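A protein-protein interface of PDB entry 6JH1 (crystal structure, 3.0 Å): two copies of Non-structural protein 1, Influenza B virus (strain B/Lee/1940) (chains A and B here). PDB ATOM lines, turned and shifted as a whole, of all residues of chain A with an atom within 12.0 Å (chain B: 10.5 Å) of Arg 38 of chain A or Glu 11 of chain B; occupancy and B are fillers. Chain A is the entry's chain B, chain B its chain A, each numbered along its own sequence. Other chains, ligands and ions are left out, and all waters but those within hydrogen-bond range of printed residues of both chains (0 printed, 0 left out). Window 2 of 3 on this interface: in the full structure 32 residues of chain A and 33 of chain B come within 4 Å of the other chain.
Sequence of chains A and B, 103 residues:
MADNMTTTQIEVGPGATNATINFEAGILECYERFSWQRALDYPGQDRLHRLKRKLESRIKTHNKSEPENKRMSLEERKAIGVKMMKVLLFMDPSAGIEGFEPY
The backbone carbonyl oxygen of Gln 9 of chain B lies within hydrogen-bond range of the side-chain amide nitrogen of Gln 45 of chain A (3.1 Å). The side-chain carboxylate (OE2) of Glu 11 of chain B is in salt-bridge range of the guanidinium group (NH2) of Arg 38 of chain A (2.9 Å). OG1 of Thr 20 of chain B lies within hydrogen-bond range of O of Ala 39 of chain A (3.1 Å). N of Asp 41 of chain A lies within hydrogen-bond range of OG1 of Thr 20 of chain B. The backbone carbonyl oxygen of Leu 88 of chain B sits at hydrogen-bond distance from the guanidinium group of Arg 33 of chain A. The backbone carbonyl oxygen of Ala 39 of chain A lies close to the backbone carbonyl oxygen of Ala 16 of chain B (3.3 Å).
O of Ala 16 of chain B lies within hydrogen-bond range of OG1 of Thr 20 of chain B (2.5 Å). O of Glu 32 of chain A sits at hydrogen-bond distance from OG of Ser 35 of chain A. O of Phe 34 of chain A sits close to OE1 of Gln 37 of chain A, 3.0 Å away. O of Leu 40 of chain A is in hydrogen-bond range of NE2 of Gln 45 of chain A, at 3.1 Å. N of Gly 44 of chain A lies within hydrogen-bond range of OD1 of Asp 41 of chain A, 3.0 Å away. A ring nitrogen (ND1) of His 49 of chain A sits at hydrogen-bond distance from the backbone carbonyl oxygen (O) of Gln 45 of chain A (2.7 Å).
CD1 of Leu 88 of chain B touches O of Cys 30 of chain A, at 3.7 Å. CA of Tyr 31 of chain A touches CZ of Phe 23 of chain B, at 3.97 Å. Ala 19 of chain B touches Phe 34 of chain A (O to CZ, 3.4 Å). Phe 34 of chain A touches Leu 88 of chain B (CA to CD1, 3.7 Å). Ile 10 of chain B touches Ser 35 of chain A (CD1 to O, 3.5 Å). CG of Arg 38 of chain A touches CG2 of Ile 10 of chain B, at 3.2 Å. CA of Val 12 of chain B touches O of Arg 38 of chain A, at 3.5 Å. Leu 40 of chain A touches Thr 20 of chain B (CD1 to CG2, 3.7 Å). Tyr 42 of chain A touches Val 12 of chain B. OE1 of Gln 9 of chain B touches CE1 of His 49 of chain A (3.995 Å).
Of chain B, only Ile 10 (3.2 Å), Glu 11 (2.9 Å) and Val 12 (3.5 Å) come within 4 Å of Arg 38 of chain A. Of the printed residues of chain B, Tyr 42 of chain A touches Val 12 (3.2 Å). Gly 44 of chain A touches none of the printed residues of chain B. Of chain A, only Ser 35 and Arg 38 come within 4 Å of Ile 10 of chain B. Glu 11 of chain B touches one residue of chain A. Of chain A, only Arg 38, Leu 40, Tyr 42 and Gln 45 come within 4 Å of Val 12 of chain B. No residue of chain A comes within 4 Å of Gly 13 of chain B. Ala 16 of chain B touches just these residues of chain A: Ala 39 (3.3 Å) and Asp 41 (3.9 Å). Of the printed residues of chain A, Thr 17 of chain B touches Asp 41. The nearest residue of chain B that does not touch Arg 38 of chain A is Gly 13 of chain B (4.2 Å).
Hydrophobic or aromatic side chains of chain B within 4 Å of the printed part of chain A: Ile 10, Val 12, Ala 16, Phe 23 and Leu 88. Along chain B the printed residues that touch a printed residue of chain A span positions 9 to 88. Hydrophobic or aromatic side chains of chain A that line the printed part of chain B: Tyr 31, Phe 34, Leu 40, Tyr 42 and His 49. Along chain A the printed residues that touch a printed residue of chain B span positions 30 to 49.
No position is printed for both chains.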
ATOM      1  N   CYS A  30      -5.560  15.593  -6.579  1.00  0.00           N
ATOM      2  CA  CYS A  30      -6.342  16.209  -5.545  1.00  0.00           C
ATOM      3  C   CYS A  30      -5.945  17.609  -5.405  1.00  0.00           C
ATOM      4  O   CYS A  30      -6.745  18.421  -5.168  1.00  0.00           O
ATOM      5  CB  CYS A  30      -6.058  15.547  -4.251  1.00  0.00           C
ATOM      6  SG  CYS A  30      -7.379  14.540  -3.670  1.00  0.00           S
ATOM      7  N   TYR A  31      -4.683  17.877  -5.533  1.00  0.00           N
ATOM      8  CA  TYR A  31      -4.212  19.199  -5.398  1.00  0.00           C
ATOM      9  C   TYR A  31      -4.780  19.987  -6.492  1.00  0.00           C
ATOM     10  O   TYR A  31      -5.481  20.926  -6.296  1.00  0.00           O
ATOM     11  CB  TYR A  31      -2.748  19.165  -5.588  1.00  0.00           C
ATOM     12  CG  TYR A  31      -1.935  19.138  -4.339  1.00  0.00           C
ATOM     13  CD1 TYR A  31      -1.461  20.276  -3.793  1.00  0.00           C
ATOM     14  CD2 TYR A  31      -1.613  17.970  -3.756  1.00  0.00           C
ATOM     15  CE1 TYR A  31      -0.703  20.243  -2.672  1.00  0.00           C
ATOM     16  CE2 TYR A  31      -0.840  17.934  -2.642  1.00  0.00           C
ATOM     17  CZ  TYR A  31      -0.396  19.078  -2.119  1.00  0.00           C
ATOM     18  OH  TYR A  31       0.359  19.040  -1.005  1.00  0.00           O
ATOM     19  N   GLU A  32      -4.513  19.541  -7.680  1.00  0.00           N
ATOM     20  CA  GLU A  32      -4.926  20.222  -8.901  1.00  0.00           C
ATOM     21  C   GLU A  32      -6.384  20.632  -8.730  1.00  0.00           C
ATOM     22  O   GLU A  32      -6.721  21.832  -8.768  1.00  0.00           O
ATOM     23  CB  GLU A  32      -4.702  19.362 -10.133  1.00  0.00           C
ATOM     24  CG  GLU A  32      -3.194  19.075 -10.319  1.00  0.00           C
ATOM     25  CD  GLU A  32      -2.823  18.492 -11.685  1.00  0.00           C
ATOM     26  OE1 GLU A  32      -3.611  17.683 -12.230  1.00  0.00           O
ATOM     27  OE2 GLU A  32      -1.728  18.833 -12.203  1.00  0.00           O
ATOM     28  N   ARG A  33      -7.253  19.651  -8.450  1.00  0.00           N
ATOM     29  CA  ARG A  33      -8.658  19.977  -8.237  1.00  0.00           C
ATOM     30  C   ARG A  33      -8.813  21.015  -7.152  1.00  0.00           C
ATOM     31  O   ARG A  33      -9.721  21.836  -7.206  1.00  0.00           O
ATOM     32  CB  ARG A  33      -9.440  18.752  -7.834  1.00  0.00           C
ATOM     33  CG  ARG A  33      -9.276  17.592  -8.730  1.00  0.00           C
ATOM     34  CD  ARG A  33     -10.474  16.744  -8.584  1.00  0.00           C
ATOM     35  NE  ARG A  33     -10.466  15.601  -9.472  1.00  0.00           N
ATOM     36  CZ  ARG A  33     -11.371  14.639  -9.408  1.00  0.00           C
ATOM     37  NH1 ARG A  33     -12.335  14.708  -8.499  1.00  0.00           N
ATOM     38  NH2 ARG A  33     -11.318  13.619 -10.246  1.00  0.00           N
ATOM     39  N   PHE A  34      -7.951  20.978  -6.145  1.00  0.00           N
ATOM     40  CA  PHE A  34      -8.028  21.961  -5.072  1.00  0.00           C
ATOM     41  C   PHE A  34      -7.742  23.372  -5.577  1.00  0.00           C
ATOM     42  O   PHE A  34      -8.537  24.296  -5.359  1.00  0.00           O
ATOM     43  CB  PHE A  34      -7.069  21.546  -3.957  1.00  0.00           C
ATOM     44  CG  PHE A  34      -7.208  22.333  -2.688  1.00  0.00           C
ATOM     45  CD1 PHE A  34      -8.431  22.485  -2.069  1.00  0.00           C
ATOM     46  CD2 PHE A  34      -6.079  22.839  -2.060  1.00  0.00           C
ATOM     47  CE1 PHE A  34      -8.524  23.196  -0.890  1.00  0.00           C
ATOM     48  CE2 PHE A  34      -6.166  23.536  -0.875  1.00  0.00           C
ATOM     49  CZ  PHE A  34      -7.382  23.722  -0.296  1.00  0.00           C
ATOM     50  N   SER A  35      -6.607  23.552  -6.263  1.00  0.00           N
ATOM     51  CA  SER A  35      -6.198  24.887  -6.687  1.00  0.00           C
ATOM     52  C   SER A  35      -7.181  25.494  -7.675  1.00  0.00           C
ATOM     53  O   SER A  35      -7.209  26.715  -7.821  1.00  0.00           O
ATOM     54  CB  SER A  35      -4.783  24.864  -7.255  1.00  0.00           C
ATOM     55  OG  SER A  35      -4.754  24.075  -8.414  1.00  0.00           O
ATOM     56  N   TRP A  36      -7.958  24.674  -8.399  1.00  0.00           N
ATOM     57  CA  TRP A  36      -9.047  25.263  -9.187  1.00  0.00           C
ATOM     58  C   TRP A  36      -9.978  26.134  -8.345  1.00  0.00           C
ATOM     59  O   TRP A  36     -10.640  27.030  -8.887  1.00  0.00           O
ATOM     60  CB  TRP A  36      -9.915  24.208  -9.855  1.00  0.00           C
ATOM     61  CG  TRP A  36      -9.216  23.366 -10.795  1.00  0.00           C
ATOM     62  CD1 TRP A  36      -8.014  23.613 -11.383  1.00  0.00           C
ATOM     63  CD2 TRP A  36      -9.655  22.087 -11.271  1.00  0.00           C
ATOM     64  NE1 TRP A  36      -7.671  22.558 -12.211  1.00  0.00           N
ATOM     65  CE2 TRP A  36      -8.660  21.608 -12.155  1.00  0.00           C
ATOM     66  CE3 TRP A  36     -10.786  21.289 -11.020  1.00  0.00           C
ATOM     67  CZ2 TRP A  36      -8.765  20.373 -12.797  1.00  0.00           C
ATOM     68  CZ3 TRP A  36     -10.894  20.063 -11.664  1.00  0.00           C
ATOM     69  CH2 TRP A  36      -9.889  19.617 -12.540  1.00  0.00           C
ATOM     70  N   GLN A  37     -10.113  25.839  -7.042  1.00  0.00           N
ATOM     71  CA  GLN A  37     -10.920  26.663  -6.138  1.00  0.00           C
ATOM     72  C   GLN A  37     -10.167  27.827  -5.580  1.00  0.00           C
ATOM     73  O   GLN A  37     -10.625  28.426  -4.595  1.00  0.00           O
ATOM     74  CB  GLN A  37     -11.473  25.847  -4.969  1.00  0.00           C
ATOM     75  CG  GLN A  37     -12.761  25.114  -5.282  1.00  0.00           C
ATOM     76  CD  GLN A  37     -12.469  23.966  -6.172  1.00  0.00           C
ATOM     77  OE1 GLN A  37     -11.326  23.547  -6.262  1.00  0.00           O
ATOM     78  NE2 GLN A  37     -13.480  23.420  -6.800  1.00  0.00           N
ATOM     79  N   ARG A  38      -9.033  28.157  -6.186  1.00  0.00           N
ATOM     80  CA  ARG A  38      -8.277  29.332  -5.796  1.00  0.00           C
ATOM     81  C   ARG A  38      -7.939  29.238  -4.312  1.00  0.00           C
ATOM     82  O   ARG A  38      -7.900  30.234  -3.585  1.00  0.00           O
ATOM     83  CB  ARG A  38      -9.073  30.607  -6.134  1.00  0.00           C
ATOM     84  CG  ARG A  38      -9.634  30.623  -7.591  1.00  0.00           C
ATOM     85  CD  ARG A  38     -10.296  31.947  -8.047  1.00  0.00           C
ATOM     86  NE  ARG A  38      -9.869  32.356  -9.402  1.00  0.00           N
ATOM     87  CZ  ARG A  38     -10.572  32.266 -10.534  1.00  0.00           C
ATOM     88  NH1 ARG A  38     -11.807  31.780 -10.533  1.00  0.00           N
ATOM     89  NH2 ARG A  38     -10.029  32.684 -11.678  1.00  0.00           N
ATOM     90  N   ALA A  39      -7.631  28.017  -3.883  1.00  0.00           N
ATOM     91  CA  ALA A  39      -7.461  27.688  -2.481  1.00  0.00           C
ATOM     92  C   ALA A  39      -6.065  27.236  -2.152  1.00  0.00           C
ATOM     93  O   ALA A  39      -5.687  27.229  -0.973  1.00  0.00           O
ATOM     94  CB  ALA A  39      -8.408  26.559  -2.068  1.00  0.00           C
ATOM     95  N   LEU A  40      -5.279  26.887  -3.147  1.00  0.00           N
ATOM     96  CA  LEU A  40      -3.938  26.431  -2.869  1.00  0.00           C
ATOM     97  C   LEU A  40      -3.064  27.649  -2.641  1.00  0.00           C
ATOM     98  O   LEU A  40      -3.026  28.556  -3.482  1.00  0.00           O
ATOM     99  CB  LEU A  40      -3.441  25.591  -4.028  1.00  0.00           C
ATOM    100  CG  LEU A  40      -2.333  24.652  -3.614  1.00  0.00           C
ATOM    101  CD1 LEU A  40      -2.843  23.942  -2.376  1.00  0.00           C
ATOM    102  CD2 LEU A  40      -2.076  23.671  -4.736  1.00  0.00           C
ATOM    103  N   ASP A  41      -2.434  27.719  -1.472  1.00  0.00           N
ATOM    104  CA  ASP A  41      -1.525  28.825  -1.216  1.00  0.00           C
ATOM    105  C   ASP A  41      -0.239  28.646  -2.043  1.00  0.00           C
ATOM    106  O   ASP A  41       0.027  27.591  -2.623  1.00  0.00           O
ATOM    107  CB  ASP A  41      -1.260  28.984   0.300  1.00  0.00           C
ATOM    108  CG  ASP A  41      -0.510  27.796   0.949  1.00  0.00           C
ATOM    109  OD1 ASP A  41       0.011  26.912   0.246  1.00  0.00           O
ATOM    110  OD2 ASP A  41      -0.437  27.760   2.207  1.00  0.00           O
ATOM    111  N   TYR A  42       0.564  29.706  -2.089  1.00  0.00           N
ATOM    112  CA  TYR A  42       1.690  29.762  -3.021  1.00  0.00           C
ATOM    113  C   TYR A  42       2.738  28.676  -2.757  1.00  0.00           C
ATOM    114  O   TYR A  42       3.119  27.962  -3.712  1.00  0.00           O
ATOM    115  CB  TYR A  42       2.260  31.189  -2.975  1.00  0.00           C
ATOM    116  CG  TYR A  42       1.286  32.259  -3.475  1.00  0.00           C
ATOM    117  CD1 TYR A  42       0.623  32.112  -4.690  1.00  0.00           C
ATOM    118  CD2 TYR A  42       0.985  33.379  -2.703  1.00  0.00           C
ATOM    119  CE1 TYR A  42      -0.263  33.066  -5.148  1.00  0.00           C
ATOM    120  CE2 TYR A  42       0.086  34.338  -3.147  1.00  0.00           C
ATOM    121  CZ  TYR A  42      -0.539  34.174  -4.372  1.00  0.00           C
ATOM    122  OH  TYR A  42      -1.443  35.114  -4.831  1.00  0.00           O
ATOM    123  N   PRO A  43       3.224  28.474  -1.522  1.00  0.00           N
ATOM    124  CA  PRO A  43       4.116  27.330  -1.280  1.00  0.00           C
ATOM    125  C   PRO A  43       3.495  26.010  -1.671  1.00  0.00           C
ATOM    126  O   PRO A  43       4.211  25.097  -2.096  1.00  0.00           O
ATOM    127  CB  PRO A  43       4.357  27.390   0.232  1.00  0.00           C
ATOM    128  CG  PRO A  43       4.164  28.799   0.580  1.00  0.00           C
ATOM    129  CD  PRO A  43       3.063  29.287  -0.301  1.00  0.00           C
ATOM    130  N   GLY A  44       2.178  25.874  -1.505  1.00  0.00           N
ATOM    131  CA  GLY A  44       1.520  24.623  -1.839  1.00  0.00           C
ATOM    132  C   GLY A  44       1.391  24.407  -3.333  1.00  0.00           C
ATOM    133  O   GLY A  44       1.541  23.286  -3.812  1.00  0.00           O
ATOM    134  N   GLN A  45       1.109  25.475  -4.090  1.00  0.00           N
ATOM    135  CA  GLN A  45       1.111  25.380  -5.550  1.00  0.00           C
ATOM    136  C   GLN A  45       2.457  24.882  -6.044  1.00  0.00           C
ATOM    137  O   GLN A  45       2.538  23.991  -6.911  1.00  0.00           O
ATOM    138  CB  GLN A  45       0.828  26.751  -6.158  1.00  0.00           C
ATOM    139  CG  GLN A  45      -0.441  27.371  -5.678  1.00  0.00           C
ATOM    140  CD  GLN A  45      -0.918  28.471  -6.572  1.00  0.00           C
ATOM    141  OE1 GLN A  45      -0.781  28.403  -7.793  1.00  0.00           O
ATOM    142  NE2 GLN A  45      -1.480  29.512  -5.970  1.00  0.00           N
ATOM    143  N   LEU A  48       2.727  21.397  -5.507  1.00  0.00           N
ATOM    144  CA  LEU A  48       2.044  20.683  -6.581  1.00  0.00           C
ATOM    145  C   LEU A  48       2.985  20.445  -7.741  1.00  0.00           C
ATOM    146  O   LEU A  48       3.034  19.348  -8.315  1.00  0.00           O
ATOM    147  CB  LEU A  48       0.844  21.493  -7.071  1.00  0.00           C
ATOM    148  CG  LEU A  48      -0.100  20.985  -8.170  1.00  0.00           C
ATOM    149  CD1 LEU A  48      -1.365  21.802  -8.147  1.00  0.00           C
ATOM    150  CD2 LEU A  48       0.490  21.040  -9.546  1.00  0.00           C
ATOM    151  N   HIS A  49       3.729  21.476  -8.118  1.00  0.00           N
ATOM    152  CA  HIS A  49       4.547  21.346  -9.311  1.00  0.00           C
ATOM    153  C   HIS A  49       5.749  20.428  -9.069  1.00  0.00           C
ATOM    154  O   HIS A  49       6.007  19.512  -9.870  1.00  0.00           O
ATOM    155  CB  HIS A  49       4.942  22.745  -9.753  1.00  0.00           C
ATOM    156  CG  HIS A  49       3.777  23.547 -10.242  1.00  0.00           C
ATOM    157  ND1 HIS A  49       3.218  24.573  -9.508  1.00  0.00           N
ATOM    158  CD2 HIS A  49       3.057  23.466 -11.387  1.00  0.00           C
ATOM    159  CE1 HIS A  49       2.205  25.092 -10.183  1.00  0.00           C
ATOM    160  NE2 HIS A  49       2.091  24.441 -11.328  1.00  0.00           N
ATOM    161  N   GLN B   9      -0.055  31.440  -8.803  1.00  0.00           N
ATOM    162  CA  GLN B   9      -1.099  31.465  -9.824  1.00  0.00           C
ATOM    163  C   GLN B   9      -2.519  31.487  -9.245  1.00  0.00           C
ATOM    164  O   GLN B   9      -2.707  31.507  -8.020  1.00  0.00           O
ATOM    165  CB  GLN B   9      -0.931  30.275 -10.771  1.00  0.00           C
ATOM    166  CG  GLN B   9       0.346  30.318 -11.605  1.00  0.00           C
ATOM    167  CD  GLN B   9       0.375  29.226 -12.649  1.00  0.00           C
ATOM    168  OE1 GLN B   9       0.619  28.062 -12.334  1.00  0.00           O
ATOM    169  NE2 GLN B   9       0.058  29.581 -13.885  1.00  0.00           N
ATOM    170  N   ILE B  10      -3.487  31.534 -10.176  1.00  0.00           N
ATOM    171  CA  ILE B  10      -4.939  31.470  -9.975  1.00  0.00           C
ATOM    172  C   ILE B  10      -5.509  32.861  -9.644  1.00  0.00           C
ATOM    173  O   ILE B  10      -5.672  33.701 -10.540  1.00  0.00           O
ATOM    174  CB  ILE B  10      -5.317  30.390  -8.929  1.00  0.00           C
ATOM    175  CG1 ILE B  10      -4.664  29.034  -9.268  1.00  0.00           C
ATOM    176  CG2 ILE B  10      -6.774  30.136  -8.947  1.00  0.00           C
ATOM    177  CD1 ILE B  10      -5.352  28.239 -10.393  1.00  0.00           C
ATOM    178  N   GLU B  11      -5.809  33.120  -8.365  1.00  0.00           N
ATOM    179  CA  GLU B  11      -6.514  34.321  -7.904  1.00  0.00           C
ATOM    180  C   GLU B  11      -6.650  34.214  -6.386  1.00  0.00           C
ATOM    181  O   GLU B  11      -7.467  34.896  -5.759  1.00  0.00           O
ATOM    182  CB  GLU B  11      -7.882  34.428  -8.593  1.00  0.00           C
ATOM    183  CG  GLU B  11      -8.738  35.683  -8.411  1.00  0.00           C
ATOM    184  CD  GLU B  11     -10.024  35.590  -9.241  1.00  0.00           C
ATOM    185  OE1 GLU B  11     -11.124  35.794  -8.675  1.00  0.00           O
ATOM    186  OE2 GLU B  11      -9.925  35.301 -10.457  1.00  0.00           O
ATOM    187  N   VAL B  12      -5.817  33.339  -5.811  1.00  0.00           N
ATOM    188  CA  VAL B  12      -5.862  32.950  -4.407  1.00  0.00           C
ATOM    189  C   VAL B  12      -5.814  34.149  -3.474  1.00  0.00           C
ATOM    190  O   VAL B  12      -4.932  35.007  -3.572  1.00  0.00           O
ATOM    191  CB  VAL B  12      -4.689  31.996  -4.160  1.00  0.00           C
ATOM    192  CG1 VAL B  12      -3.453  32.625  -4.673  1.00  0.00           C
ATOM    193  CG2 VAL B  12      -4.465  31.846  -2.727  1.00  0.00           C
ATOM    194  N   GLY B  13      -6.738  34.173  -2.517  1.00  0.00           N
ATOM    195  CA  GLY B  13      -6.818  35.229  -1.534  1.00  0.00           C
ATOM    196  C   GLY B  13      -6.230  34.866  -0.184  1.00  0.00           C
ATOM    197  O   GLY B  13      -5.552  33.845  -0.016  1.00  0.00           O
ATOM    198  N   PRO B  14      -6.492  35.704   0.819  1.00  0.00           N
ATOM    199  CA  PRO B  14      -6.077  35.358   2.179  1.00  0.00           C
ATOM    200  C   PRO B  14      -6.878  34.156   2.633  1.00  0.00           C
ATOM    201  O   PRO B  14      -7.902  33.797   2.041  1.00  0.00           O
ATOM    202  CB  PRO B  14      -6.429  36.601   3.006  1.00  0.00           C
ATOM    203  CG  PRO B  14      -7.525  37.265   2.250  1.00  0.00           C
ATOM    204  CD  PRO B  14      -7.386  36.881   0.790  1.00  0.00           C
ATOM    205  N   GLY B  15      -6.403  33.506   3.680  1.00  0.00           N
ATOM    206  CA  GLY B  15      -7.157  32.346   4.106  1.00  0.00           C
ATOM    207  C   GLY B  15      -7.067  31.163   3.171  1.00  0.00           C
ATOM    208  O   GLY B  15      -7.760  30.166   3.381  1.00  0.00           O
ATOM    209  N   ALA B  16      -6.277  31.260   2.116  1.00  0.00           N
ATOM    210  CA  ALA B  16      -5.880  30.053   1.417  1.00  0.00           C
ATOM    211  C   ALA B  16      -4.814  29.313   2.198  1.00  0.00           C
ATOM    212  O   ALA B  16      -4.648  28.109   2.004  1.00  0.00           O
ATOM    213  CB  ALA B  16      -5.370  30.376   0.021  1.00  0.00           C
ATOM    214  N   THR B  17      -4.023  30.043   2.993  1.00  0.00           N
ATOM    215  CA  THR B  17      -3.067  29.421   3.904  1.00  0.00           C
ATOM    216  C   THR B  17      -3.770  28.516   4.918  1.00  0.00           C
ATOM    217  O   THR B  17      -3.345  27.375   5.143  1.00  0.00           O
ATOM    218  CB  THR B  17      -2.264  30.503   4.617  1.00  0.00           C
ATOM    219  OG1 THR B  17      -3.171  31.448   5.188  1.00  0.00           O
ATOM    220  CG2 THR B  17      -1.361  31.224   3.640  1.00  0.00           C
ATOM    221  N   ASN B  18      -4.860  28.993   5.532  1.00  0.00           N
ATOM    222  CA  ASN B  18      -5.585  28.124   6.456  1.00  0.00           C
ATOM    223  C   ASN B  18      -6.125  26.896   5.729  1.00  0.00           C
ATOM    224  O   ASN B  18      -5.930  25.764   6.177  1.00  0.00           O
ATOM    225  CB  ASN B  18      -6.711  28.884   7.161  1.00  0.00           C
ATOM    226  CG  ASN B  18      -7.560  27.970   8.082  1.00  0.00           C
ATOM    227  OD1 ASN B  18      -7.047  27.010   8.654  1.00  0.00           O
ATOM    228  ND2 ASN B  18      -8.818  28.332   8.303  1.00  0.00           N
ATOM    229  N   ALA B  19      -6.791  27.094   4.587  1.00  0.00           N
ATOM    230  CA  ALA B  19      -7.327  25.962   3.834  1.00  0.00           C
ATOM    231  C   ALA B  19      -6.251  25.062   3.257  1.00  0.00           C
ATOM    232  O   ALA B  19      -6.536  23.907   2.942  1.00  0.00           O
ATOM    233  CB  ALA B  19      -8.232  26.438   2.709  1.00  0.00           C
ATOM    234  N   THR B  20      -5.032  25.545   3.078  1.00  0.00           N
ATOM    235  CA  THR B  20      -3.988  24.623   2.655  1.00  0.00           C
ATOM    236  C   THR B  20      -3.437  23.832   3.828  1.00  0.00           C
ATOM    237  O   THR B  20      -3.145  22.644   3.685  1.00  0.00           O
ATOM    238  CB  THR B  20      -2.902  25.372   1.916  1.00  0.00           C
ATOM    239  OG1 THR B  20      -3.532  26.177   0.919  1.00  0.00           O
ATOM    240  CG2 THR B  20      -1.987  24.401   1.230  1.00  0.00           C
ATOM    241  N   PHE B  23      -6.054  21.280   4.048  1.00  0.00           N
ATOM    242  CA  PHE B  23      -6.060  20.363   2.984  1.00  0.00           C
ATOM    243  C   PHE B  23      -4.993  19.368   3.226  1.00  0.00           C
ATOM    244  O   PHE B  23      -5.219  18.217   3.133  1.00  0.00           O
ATOM    245  CB  PHE B  23      -5.779  21.122   1.738  1.00  0.00           C
ATOM    246  CG  PHE B  23      -5.661  20.283   0.546  1.00  0.00           C
ATOM    247  CD1 PHE B  23      -6.729  19.616   0.083  1.00  0.00           C
ATOM    248  CD2 PHE B  23      -4.490  20.192  -0.114  1.00  0.00           C
ATOM    249  CE1 PHE B  23      -6.629  18.840  -1.013  1.00  0.00           C
ATOM    250  CE2 PHE B  23      -4.379  19.424  -1.212  1.00  0.00           C
ATOM    251  CZ  PHE B  23      -5.447  18.744  -1.653  1.00  0.00           C
ATOM    252  N   LEU B  88     -13.863  17.078  -3.078  1.00  0.00           N
ATOM    253  CA  LEU B  88     -13.136  17.201  -4.341  1.00  0.00           C
ATOM    254  C   LEU B  88     -13.218  15.922  -5.157  1.00  0.00           C
ATOM    255  O   LEU B  88     -13.374  15.966  -6.382  1.00  0.00           O
ATOM    256  CB  LEU B  88     -11.665  17.552  -4.100  1.00  0.00           C
ATOM    257  CG  LEU B  88     -11.423  18.979  -3.623  1.00  0.00           C
ATOM    258  CD1 LEU B  88      -9.948  19.238  -3.575  1.00  0.00           C
ATOM    259  CD2 LEU B  88     -12.150  19.986  -4.516  1.00  0.00           C
